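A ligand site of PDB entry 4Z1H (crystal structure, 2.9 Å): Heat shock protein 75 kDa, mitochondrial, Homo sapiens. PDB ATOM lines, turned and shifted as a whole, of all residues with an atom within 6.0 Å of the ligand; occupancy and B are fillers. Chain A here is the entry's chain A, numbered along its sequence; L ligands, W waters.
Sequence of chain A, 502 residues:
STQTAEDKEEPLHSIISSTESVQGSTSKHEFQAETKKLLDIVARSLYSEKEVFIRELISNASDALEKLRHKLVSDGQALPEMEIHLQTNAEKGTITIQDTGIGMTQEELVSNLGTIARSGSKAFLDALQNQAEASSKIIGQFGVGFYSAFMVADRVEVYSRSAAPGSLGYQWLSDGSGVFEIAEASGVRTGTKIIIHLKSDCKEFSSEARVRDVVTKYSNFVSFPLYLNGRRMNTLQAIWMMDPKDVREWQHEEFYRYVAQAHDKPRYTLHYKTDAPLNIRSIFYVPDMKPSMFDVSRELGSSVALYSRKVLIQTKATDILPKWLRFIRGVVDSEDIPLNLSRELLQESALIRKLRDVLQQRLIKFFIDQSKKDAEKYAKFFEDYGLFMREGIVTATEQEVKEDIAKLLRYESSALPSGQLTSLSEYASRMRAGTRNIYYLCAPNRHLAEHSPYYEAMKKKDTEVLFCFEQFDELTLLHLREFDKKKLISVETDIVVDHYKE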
ATOM      1  N   LEU A  57     -38.695 -13.696  -0.981  1.00  0.00           N
ATOM      2  CA  LEU A  57     -37.620 -14.341  -1.734  1.00  0.00           C
ATOM      3  C   LEU A  57     -37.120 -13.426  -2.857  1.00  0.00           C
ATOM      4  O   LEU A  57     -35.908 -13.240  -3.018  1.00  0.00           O
ATOM      5  CB  LEU A  57     -38.091 -15.674  -2.307  1.00  0.00           C
ATOM      6  CG  LEU A  57     -38.411 -16.791  -1.309  1.00  0.00           C
ATOM      7  CD1 LEU A  57     -38.867 -18.046  -2.019  1.00  0.00           C
ATOM      8  CD2 LEU A  57     -37.233 -17.081  -0.418  1.00  0.00           C
ATOM      9  N   ASN A  60     -34.920 -10.766  -1.345  1.00  0.00           N
ATOM     10  CA  ASN A  60     -33.570 -11.255  -1.111  1.00  0.00           C
ATOM     11  C   ASN A  60     -32.747 -11.373  -2.396  1.00  0.00           C
ATOM     12  O   ASN A  60     -31.569 -11.017  -2.421  1.00  0.00           O
ATOM     13  CB  ASN A  60     -33.601 -12.624  -0.406  1.00  0.00           C
ATOM     14  CG  ASN A  60     -34.089 -12.529   1.020  1.00  0.00           C
ATOM     15  OD1 ASN A  60     -33.946 -11.502   1.677  1.00  0.00           O
ATOM     16  ND2 ASN A  60     -34.656 -13.624   1.513  1.00  0.00           N
ATOM     17  N   ALA A  61     -33.378 -11.876  -3.460  1.00  0.00           N
ATOM     18  CA  ALA A  61     -32.713 -11.957  -4.756  1.00  0.00           C
ATOM     19  C   ALA A  61     -32.286 -10.571  -5.247  1.00  0.00           C
ATOM     20  O   ALA A  61     -31.186 -10.395  -5.792  1.00  0.00           O
ATOM     21  CB  ALA A  61     -33.627 -12.604  -5.777  1.00  0.00           C
ATOM     22  N   ALA A  64     -29.293  -9.372  -3.223  1.00  0.00           N
ATOM     23  CA  ALA A  64     -28.124 -10.132  -3.675  1.00  0.00           C
ATOM     24  C   ALA A  64     -27.572  -9.574  -4.984  1.00  0.00           C
ATOM     25  O   ALA A  64     -26.360  -9.310  -5.098  1.00  0.00           O
ATOM     26  CB  ALA A  64     -28.490 -11.598  -3.852  1.00  0.00           C
ATOM     27  N   ASP A  99     -31.436 -16.540  -8.743  1.00  0.00           N
ATOM     28  CA  ASP A  99     -30.890 -15.220  -9.018  1.00  0.00           C
ATOM     29  C   ASP A  99     -29.413 -15.324  -9.321  1.00  0.00           C
ATOM     30  O   ASP A  99     -28.687 -16.126  -8.697  1.00  0.00           O
ATOM     31  CB  ASP A  99     -31.136 -14.280  -7.832  1.00  0.00           C
ATOM     32  CG  ASP A  99     -30.513 -14.778  -6.560  1.00  0.00           C
ATOM     33  OD1 ASP A  99     -29.305 -14.534  -6.347  1.00  0.00           O
ATOM     34  OD2 ASP A  99     -31.215 -15.410  -5.757  1.00  0.00           O
ATOM     35  N   ILE A 102     -24.996 -11.992  -6.038  1.00  0.00           N
ATOM     36  CA  ILE A 102     -23.915 -12.456  -5.187  1.00  0.00           C
ATOM     37  C   ILE A 102     -24.457 -13.709  -4.511  1.00  0.00           C
ATOM     38  O   ILE A 102     -25.669 -13.876  -4.387  1.00  0.00           O
ATOM     39  CB  ILE A 102     -23.500 -11.384  -4.146  1.00  0.00           C
ATOM     40  CG1 ILE A 102     -21.992 -11.434  -3.887  1.00  0.00           C
ATOM     41  CG2 ILE A 102     -24.286 -11.526  -2.854  1.00  0.00           C
ATOM     42  CD1 ILE A 102     -21.453 -10.217  -3.153  1.00  0.00           C
ATOM     43  N   GLY A 103     -23.565 -14.599  -4.098  1.00  0.00           N
ATOM     44  CA  GLY A 103     -24.037 -15.858  -3.538  1.00  0.00           C
ATOM     45  C   GLY A 103     -23.886 -15.914  -2.032  1.00  0.00           C
ATOM     46  O   GLY A 103     -23.885 -14.892  -1.361  1.00  0.00           O
ATOM     47  N   MET A 104     -23.774 -17.135  -1.506  1.00  0.00           N
ATOM     48  CA  MET A 104     -23.492 -17.331  -0.098  1.00  0.00           C
ATOM     49  C   MET A 104     -22.288 -18.251   0.067  1.00  0.00           C
ATOM     50  O   MET A 104     -22.174 -19.265  -0.627  1.00  0.00           O
ATOM     51  CB  MET A 104     -24.711 -17.916   0.625  1.00  0.00           C
ATOM     52  CG  MET A 104     -25.812 -16.918   0.886  1.00  0.00           C
ATOM     53  SD  MET A 104     -27.260 -17.664   1.655  1.00  0.00           S
ATOM     54  CE  MET A 104     -27.850 -18.673   0.288  1.00  0.00           C
ATOM     55  N   GLU A 107     -19.708 -20.526   5.087  1.00  0.00           N
ATOM     56  CA  GLU A 107     -19.819 -19.921   6.409  1.00  0.00           C
ATOM     57  C   GLU A 107     -21.206 -19.299   6.625  1.00  0.00           C
ATOM     58  O   GLU A 107     -21.804 -19.439   7.704  1.00  0.00           O
ATOM     59  CB  GLU A 107     -18.730 -18.866   6.594  1.00  0.00           C
ATOM     60  CG  GLU A 107     -18.774 -18.095   7.905  1.00  0.00           C
ATOM     61  CD  GLU A 107     -17.642 -17.100   8.049  1.00  0.00           C
ATOM     62  OE1 GLU A 107     -17.624 -16.089   7.302  1.00  0.00           O
ATOM     63  OE2 GLU A 107     -16.752 -17.318   8.903  1.00  0.00           O
ATOM     64  N   GLU A 108     -21.714 -18.638   5.589  1.00  0.00           N
ATOM     65  CA  GLU A 108     -23.019 -17.988   5.640  1.00  0.00           C
ATOM     66  C   GLU A 108     -24.140 -19.021   5.651  1.00  0.00           C
ATOM     67  O   GLU A 108     -25.056 -18.929   6.474  1.00  0.00           O
ATOM     68  CB  GLU A 108     -23.170 -17.029   4.448  1.00  0.00           C
ATOM     69  CG  GLU A 108     -22.144 -15.895   4.446  1.00  0.00           C
ATOM     70  CD  GLU A 108     -22.133 -15.121   3.157  1.00  0.00           C
ATOM     71  OE1 GLU A 108     -23.027 -15.343   2.313  1.00  0.00           O
ATOM     72  OE2 GLU A 108     -21.220 -14.280   2.966  1.00  0.00           O
ATOM     73  N   LEU A 109     -24.071 -19.992   4.756  1.00  0.00           N
ATOM     74  CA  LEU A 109     -25.072 -21.059   4.686  1.00  0.00           C
ATOM     75  C   LEU A 109     -25.176 -21.817   6.017  1.00  0.00           C
ATOM     76  O   LEU A 109     -26.279 -22.135   6.474  1.00  0.00           O
ATOM     77  CB  LEU A 109     -24.738 -22.040   3.561  1.00  0.00           C
ATOM     78  CG  LEU A 109     -25.181 -21.649   2.148  1.00  0.00           C
ATOM     79  CD1 LEU A 109     -24.634 -22.625   1.119  1.00  0.00           C
ATOM     80  CD2 LEU A 109     -26.693 -21.610   2.089  1.00  0.00           C
ATOM     81  N   SER A 111     -24.099 -20.615   9.071  1.00  0.00           N
ATOM     82  CA  SER A 111     -24.633 -19.653  10.036  1.00  0.00           C
ATOM     83  C   SER A 111     -26.100 -19.356   9.753  1.00  0.00           C
ATOM     84  O   SER A 111     -27.001 -19.857  10.430  1.00  0.00           O
ATOM     85  CB  SER A 111     -23.837 -18.357  10.001  1.00  0.00           C
ATOM     86  OG  SER A 111     -24.137 -17.636   8.832  1.00  0.00           O
ATOM     87  N   ASN A 112     -26.322 -18.535   8.723  1.00  0.00           N
ATOM     88  CA  ASN A 112     -27.654 -18.102   8.342  1.00  0.00           C
ATOM     89  C   ASN A 112     -28.557 -19.271   7.973  1.00  0.00           C
ATOM     90  O   ASN A 112     -29.718 -19.333   8.370  1.00  0.00           O
ATOM     91  CB  ASN A 112     -27.572 -17.130   7.164  1.00  0.00           C
ATOM     92  CG  ASN A 112     -26.559 -16.029   7.403  1.00  0.00           C
ATOM     93  OD1 ASN A 112     -25.607 -15.880   6.646  1.00  0.00           O
ATOM     94  ND2 ASN A 112     -26.759 -15.269   8.470  1.00  0.00           N
ATOM     95  N   PHE A 142     -33.936  -9.667   5.382  1.00  0.00           N
ATOM     96  CA  PHE A 142     -32.558  -9.272   5.673  1.00  0.00           C
ATOM     97  C   PHE A 142     -31.840 -10.108   6.765  1.00  0.00           C
ATOM     98  O   PHE A 142     -31.234  -9.539   7.670  1.00  0.00           O
ATOM     99  CB  PHE A 142     -32.551  -7.785   6.063  1.00  0.00           C
ATOM    100  CG  PHE A 142     -33.396  -7.459   7.276  1.00  0.00           C
ATOM    101  CD1 PHE A 142     -32.818  -7.319   8.525  1.00  0.00           C
ATOM    102  CD2 PHE A 142     -34.776  -7.338   7.167  1.00  0.00           C
ATOM    103  CE1 PHE A 142     -33.583  -7.034   9.643  1.00  0.00           C
ATOM    104  CE2 PHE A 142     -35.556  -7.054   8.276  1.00  0.00           C
ATOM    105  CZ  PHE A 142     -34.952  -6.904   9.514  1.00  0.00           C
ATOM    106  N   GLY A 143     -31.864 -11.440   6.674  1.00  0.00           N
ATOM    107  CA  GLY A 143     -32.467 -12.193   5.576  1.00  0.00           C
ATOM    108  C   GLY A 143     -33.539 -13.179   6.019  1.00  0.00           C
ATOM    109  O   GLY A 143     -33.841 -14.131   5.303  1.00  0.00           O
ATOM    110  N   VAL A 144     -34.140 -12.933   7.184  1.00  0.00           N
ATOM    111  CA  VAL A 144     -35.125 -13.835   7.775  1.00  0.00           C
ATOM    112  C   VAL A 144     -36.267 -14.225   6.840  1.00  0.00           C
ATOM    113  O   VAL A 144     -36.796 -15.346   6.934  1.00  0.00           O
ATOM    114  CB  VAL A 144     -35.726 -13.217   9.047  1.00  0.00           C
ATOM    115  CG1 VAL A 144     -36.474 -14.282   9.851  1.00  0.00           C
ATOM    116  CG2 VAL A 144     -34.634 -12.615   9.900  1.00  0.00           C
ATOM    117  N   GLY A 145     -36.633 -13.327   5.928  1.00  0.00           N
ATOM    118  CA  GLY A 145     -37.669 -13.574   4.943  1.00  0.00           C
ATOM    119  C   GLY A 145     -37.633 -14.953   4.294  1.00  0.00           C
ATOM    120  O   GLY A 145     -38.677 -15.517   3.999  1.00  0.00           O
ATOM    121  N   PHE A 146     -36.430 -15.475   4.068  1.00  0.00           N
ATOM    122  CA  PHE A 146     -36.261 -16.800   3.483  1.00  0.00           C
ATOM    123  C   PHE A 146     -37.103 -17.875   4.164  1.00  0.00           C
ATOM    124  O   PHE A 146     -37.722 -18.694   3.484  1.00  0.00           O
ATOM    125  CB  PHE A 146     -34.779 -17.198   3.540  1.00  0.00           C
ATOM    126  CG  PHE A 146     -34.531 -18.658   3.259  1.00  0.00           C
ATOM    127  CD1 PHE A 146     -34.553 -19.143   1.953  1.00  0.00           C
ATOM    128  CD2 PHE A 146     -34.246 -19.540   4.295  1.00  0.00           C
ATOM    129  CE1 PHE A 146     -34.316 -20.491   1.698  1.00  0.00           C
ATOM    130  CE2 PHE A 146     -34.016 -20.886   4.052  1.00  0.00           C
ATOM    131  CZ  PHE A 146     -34.056 -21.354   2.749  1.00  0.00           C
ATOM    132  N   TYR A 147     -37.151 -17.853   5.494  1.00  0.00           N
ATOM    133  CA  TYR A 147     -37.828 -18.914   6.223  1.00  0.00           C
ATOM    134  C   TYR A 147     -39.339 -18.900   5.976  1.00  0.00           C
ATOM    135  O   TYR A 147     -40.024 -19.875   6.277  1.00  0.00           O
ATOM    136  CB  TYR A 147     -37.511 -18.820   7.714  1.00  0.00           C
ATOM    137  CG  TYR A 147     -36.051 -19.091   8.005  1.00  0.00           C
ATOM    138  CD1 TYR A 147     -35.206 -18.076   8.423  1.00  0.00           C
ATOM    139  CD2 TYR A 147     -35.511 -20.360   7.829  1.00  0.00           C
ATOM    140  CE1 TYR A 147     -33.863 -18.322   8.680  1.00  0.00           C
ATOM    141  CE2 TYR A 147     -34.174 -20.603   8.074  1.00  0.00           C
ATOM    142  CZ  TYR A 147     -33.358 -19.585   8.507  1.00  0.00           C
ATOM    143  OH  TYR A 147     -32.031 -19.838   8.747  1.00  0.00           O
ATOM    144  N   VAL A 158     -31.873 -25.847  -1.720  1.00  0.00           N
ATOM    145  CA  VAL A 158     -31.200 -24.617  -2.137  1.00  0.00           C
ATOM    146  C   VAL A 158     -29.787 -24.878  -2.629  1.00  0.00           C
ATOM    147  O   VAL A 158     -29.001 -25.554  -1.965  1.00  0.00           O
ATOM    148  CB  VAL A 158     -31.149 -23.605  -0.974  1.00  0.00           C
ATOM    149  CG1 VAL A 158     -30.348 -22.362  -1.373  1.00  0.00           C
ATOM    150  CG2 VAL A 158     -32.542 -23.216  -0.557  1.00  0.00           C
ATOM    151  N   SER A 160     -26.324 -22.778  -3.834  1.00  0.00           N
ATOM    152  CA  SER A 160     -25.764 -21.428  -3.854  1.00  0.00           C
ATOM    153  C   SER A 160     -24.265 -21.444  -4.049  1.00  0.00           C
ATOM    154  O   SER A 160     -23.557 -22.264  -3.459  1.00  0.00           O
ATOM    155  CB  SER A 160     -26.124 -20.673  -2.565  1.00  0.00           C
ATOM    156  OG  SER A 160     -25.761 -19.301  -2.676  1.00  0.00           O
ATOM    157  N   TRP A 172     -28.062 -27.217   0.150  1.00  0.00           N
ATOM    158  CA  TRP A 172     -28.637 -26.965   1.463  1.00  0.00           C
ATOM    159  C   TRP A 172     -30.051 -27.532   1.471  1.00  0.00           C
ATOM    160  O   TRP A 172     -30.885 -27.102   0.675  1.00  0.00           O
ATOM    161  CB  TRP A 172     -28.640 -25.454   1.743  1.00  0.00           C
ATOM    162  CG  TRP A 172     -29.062 -25.081   3.123  1.00  0.00           C
ATOM    163  CD1 TRP A 172     -28.259 -24.789   4.175  1.00  0.00           C
ATOM    164  CD2 TRP A 172     -30.415 -24.936   3.595  1.00  0.00           C
ATOM    165  NE1 TRP A 172     -29.011 -24.464   5.278  1.00  0.00           N
ATOM    166  CE2 TRP A 172     -30.343 -24.552   4.948  1.00  0.00           C
ATOM    167  CE3 TRP A 172     -31.677 -25.093   3.010  1.00  0.00           C
ATOM    168  CZ2 TRP A 172     -31.484 -24.329   5.721  1.00  0.00           C
ATOM    169  CZ3 TRP A 172     -32.795 -24.871   3.780  1.00  0.00           C
ATOM    170  CH2 TRP A 172     -32.694 -24.489   5.117  1.00  0.00           C
ATOM    171  N   GLY A 191     -24.677 -17.208  -7.723  1.00  0.00           N
ATOM    172  CA  GLY A 191     -25.991 -16.759  -7.310  1.00  0.00           C
ATOM    173  C   GLY A 191     -26.723 -17.851  -6.575  1.00  0.00           C
ATOM    174  O   GLY A 191     -26.163 -18.931  -6.335  1.00  0.00           O
ATOM    175  N   THR A 192     -27.980 -17.606  -6.220  1.00  0.00           N
ATOM    176  CA  THR A 192     -28.696 -18.561  -5.372  1.00  0.00           C
ATOM    177  C   THR A 192     -29.879 -19.174  -6.095  1.00  0.00           C
ATOM    178  O   THR A 192     -30.635 -18.476  -6.778  1.00  0.00           O
ATOM    179  CB  THR A 192     -29.188 -17.875  -4.078  1.00  0.00           C
ATOM    180  OG1 THR A 192     -28.065 -17.315  -3.384  1.00  0.00           O
ATOM    181  CG2 THR A 192     -29.872 -18.889  -3.185  1.00  0.00           C
ATOM    182  N   ILE A 194     -33.277 -21.477  -5.285  1.00  0.00           N
ATOM    183  CA  ILE A 194     -34.123 -22.010  -4.234  1.00  0.00           C
ATOM    184  C   ILE A 194     -35.299 -22.799  -4.807  1.00  0.00           C
ATOM    185  O   ILE A 194     -36.155 -22.233  -5.496  1.00  0.00           O
ATOM    186  CB  ILE A 194     -34.669 -20.880  -3.329  1.00  0.00           C
ATOM    187  CG1 ILE A 194     -33.504 -20.101  -2.712  1.00  0.00           C
ATOM    188  CG2 ILE A 194     -35.567 -21.435  -2.232  1.00  0.00           C
ATOM    189  CD1 ILE A 194     -33.949 -18.959  -1.831  1.00  0.00           C
HETATM  190  C1  LIG L   1     -29.848 -14.910  -1.701  1.00  0.00           C
HETATM  191  C2  LIG L   1     -27.597 -14.382  -1.300  1.00  0.00           C
HETATM  192  N1  LIG L   1     -30.911 -15.186  -2.614  1.00  0.00           N
HETATM  193  N2  LIG L   1     -28.601 -14.649  -2.145  1.00  0.00           N
HETATM  194  N3  LIG L   1     -27.744 -14.371   0.030  1.00  0.00           N
HETATM  195  C3  LIG L   1     -30.784 -14.978   1.820  1.00  0.00           C
HETATM  196  C4  LIG L   1     -30.067 -14.903  -0.272  1.00  0.00           C
HETATM  197  C5  LIG L   1     -28.980 -14.627   0.589  1.00  0.00           C
HETATM  198  N4  LIG L   1     -31.177 -15.126   0.534  1.00  0.00           N
HETATM  199  N5  LIG L   1     -29.476 -14.695   1.894  1.00  0.00           N
HETATM  200  S1  LIG L   1     -31.815 -15.180   3.239  1.00  0.00           S
HETATM  201  C6  LIG L   1     -30.491 -18.336   5.470  1.00  0.00           C
HETATM  202  C7  LIG L   1     -30.905 -17.039   5.125  1.00  0.00           C
HETATM  203  C8  LIG L   1     -31.292 -16.789   3.794  1.00  0.00           C
HETATM  204  C9  LIG L   1     -31.262 -17.800   2.823  1.00  0.00           C
HETATM  205  I1  LIG L   1     -30.913 -15.553   6.626  1.00  0.00           I
HETATM  206  C10 LIG L   1     -30.850 -19.103   3.185  1.00  0.00           C
HETATM  207  C11 LIG L   1     -30.468 -19.370   4.490  1.00  0.00           C
HETATM  208  O1  LIG L   1     -30.114 -20.732   4.551  1.00  0.00           O
HETATM  209  O2  LIG L   1     -30.713 -20.306   2.478  1.00  0.00           O
HETATM  210  C12 LIG L   1     -30.280 -21.235   3.328  1.00  0.00           C
HETATM  211  C13 LIG L   1     -28.712 -14.460   3.100  1.00  0.00           C
HETATM  212  C14 LIG L   1     -27.975 -13.096   3.019  1.00  0.00           C
HETATM  213  C15 LIG L   1     -28.338 -12.175   4.211  1.00  0.00           C
HETATM  214  C16 LIG L   1     -26.283 -11.918   5.724  1.00  0.00           C
HETATM  215  C17 LIG L   1     -25.123 -12.884   6.095  1.00  0.00           C
HETATM  216  C18 LIG L   1     -27.645 -12.634   5.520  1.00  0.00           C
HETATM  217  C19 LIG L   1     -21.576 -15.252   9.731  1.00  0.00           C
HETATM  218  C20 LIG L   1     -22.075 -15.573   8.467  1.00  0.00           C
HETATM  219  C21 LIG L   1     -22.850 -14.651   7.761  1.00  0.00           C
HETATM  220  C22 LIG L   1     -23.111 -13.388   8.316  1.00  0.00           C
HETATM  221  C23 LIG L   1     -22.598 -13.071   9.581  1.00  0.00           C
HETATM  222  C24 LIG L   1     -21.832 -13.997  10.291  1.00  0.00           C
HETATM  223  C25 LIG L   1     -21.568  -8.859   5.269  1.00  0.00           C
HETATM  224  C26 LIG L   1     -22.915  -8.601   5.559  1.00  0.00           C
HETATM  225  C27 LIG L   1     -23.692  -9.563   6.204  1.00  0.00           C
HETATM  226  C28 LIG L   1     -23.135 -10.778   6.581  1.00  0.00           C
HETATM  227  C29 LIG L   1     -21.788 -11.036   6.291  1.00  0.00           C
HETATM  228  C30 LIG L   1     -21.000 -10.083   5.639  1.00  0.00           C
HETATM  229  P1  LIG L   1     -24.106 -12.102   7.433  1.00  0.00           P
HETATM  230  C31 LIG L   1     -27.081 -10.542  10.667  1.00  0.00           C
HETATM  231  C32 LIG L   1     -26.213  -9.640  10.046  1.00  0.00           C
HETATM  232  C33 LIG L   1     -25.302 -10.077   9.076  1.00  0.00           C
HETATM  233  C34 LIG L   1     -25.278 -11.435   8.717  1.00  0.00           C
HETATM  234  C35 LIG L   1     -26.151 -12.330   9.334  1.00  0.00           C
HETATM  235  C36 LIG L   1     -27.056 -11.895  10.316  1.00  0.00           C
HETATM  236  O   HOH W   1     -33.952 -15.862  -0.044  1.00  0.00           O
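N2 of the ligand lies within hydrogen-bond range of OG1 of Thr 192 (3.0 Å).
The side-chain carboxylate of Asp 99 is in hydrogen-bond range of a nitrogen (N1) of the ligand.
The side-chain amide nitrogen (ND2) of Asn 60 lies close to a sulfur (S1) of the ligand (3.7 Å).
The side-chain hydroxyl (OG) of Ser 111 sits at hydrogen-bond distance from the backbone carbonyl oxygen (O) of Glu 108, at 2.8 Å.
The backbone carbonyl oxygen (O) of Glu 107 sits at hydrogen-bond distance from the side-chain hydroxyl (OG) of Ser 111, 3.2 Å away.
The backbone NH (N) of Asp 99 is in hydrogen-bond range of the backbone carbonyl oxygen (O) of Thr 192 (2.9 Å).
The side-chain hydroxyl (OG1) of Thr 192 is in hydrogen-bond range of the side-chain hydroxyl (OG) of Ser 160 (3.1 Å).
The side-chain amide oxygen (OD1) of Asn 112 sits close to the backbone carbonyl oxygen (O) of Glu 108 (3.1 Å).
The side-chain hydroxyl of Ser 160 sits at hydrogen-bond distance from the backbone NH of Met 104 (3.2 Å).
The backbone carbonyl oxygen of Ala 64 lies within hydrogen-bond range of the backbone NH of Ile 102 (3.2 Å).
The backbone NH (N) of Trp 172 lies within hydrogen-bond range of the backbone carbonyl oxygen (O) of Val 158 (2.8 Å).
The side-chain sulfur of Met 104 sits close to a nitrogen (N3) of the ligand (3.7 Å).
The backbone carbonyl oxygen of Gly 143 sits close to a sulfur (S1) of the ligand (3.1 Å).
CB of Ala 64 touches N2 of the ligand (3.5 Å).
Ile 102 touches the ligand (O to C2, 3.7 Å).
O of Gly 103 touches C2 of the ligand, 3.7 Å away.
Glu 107 touches the ligand.
Glu 108 touches the ligand (CG to C21, 3.6 Å).
Leu 109 touches the ligand.
Ser 111 touches the ligand.
Asn 112 touches the ligand.
CG of Phe 146 touches C9 of the ligand (3.4 Å).
Tyr 147 touches the ligand.
Trp 172 touches the ligand (CE2 to C12, 3.7 Å).
Hydrophobic or aromatic side chains that line the ligand: Ala 64, Met 104, Leu 109, Phe 146 and Trp 172.
16 residues have an atom within 4 Å of the ligand: Asn 60, Ala 64, Asp 99, Ile 102, Gly 103, Met 104, Glu 107, Glu 108, Leu 109, Ser 111, Asn 112, Gly 143, Phe 146, Tyr 147, Trp 172 and Thr 192.
Water W1 bridges the side-chain amide nitrogen (ND2) of Asn 60 (2.8 Å) and a nitrogen (N4) of the ligand (2.9 Å).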
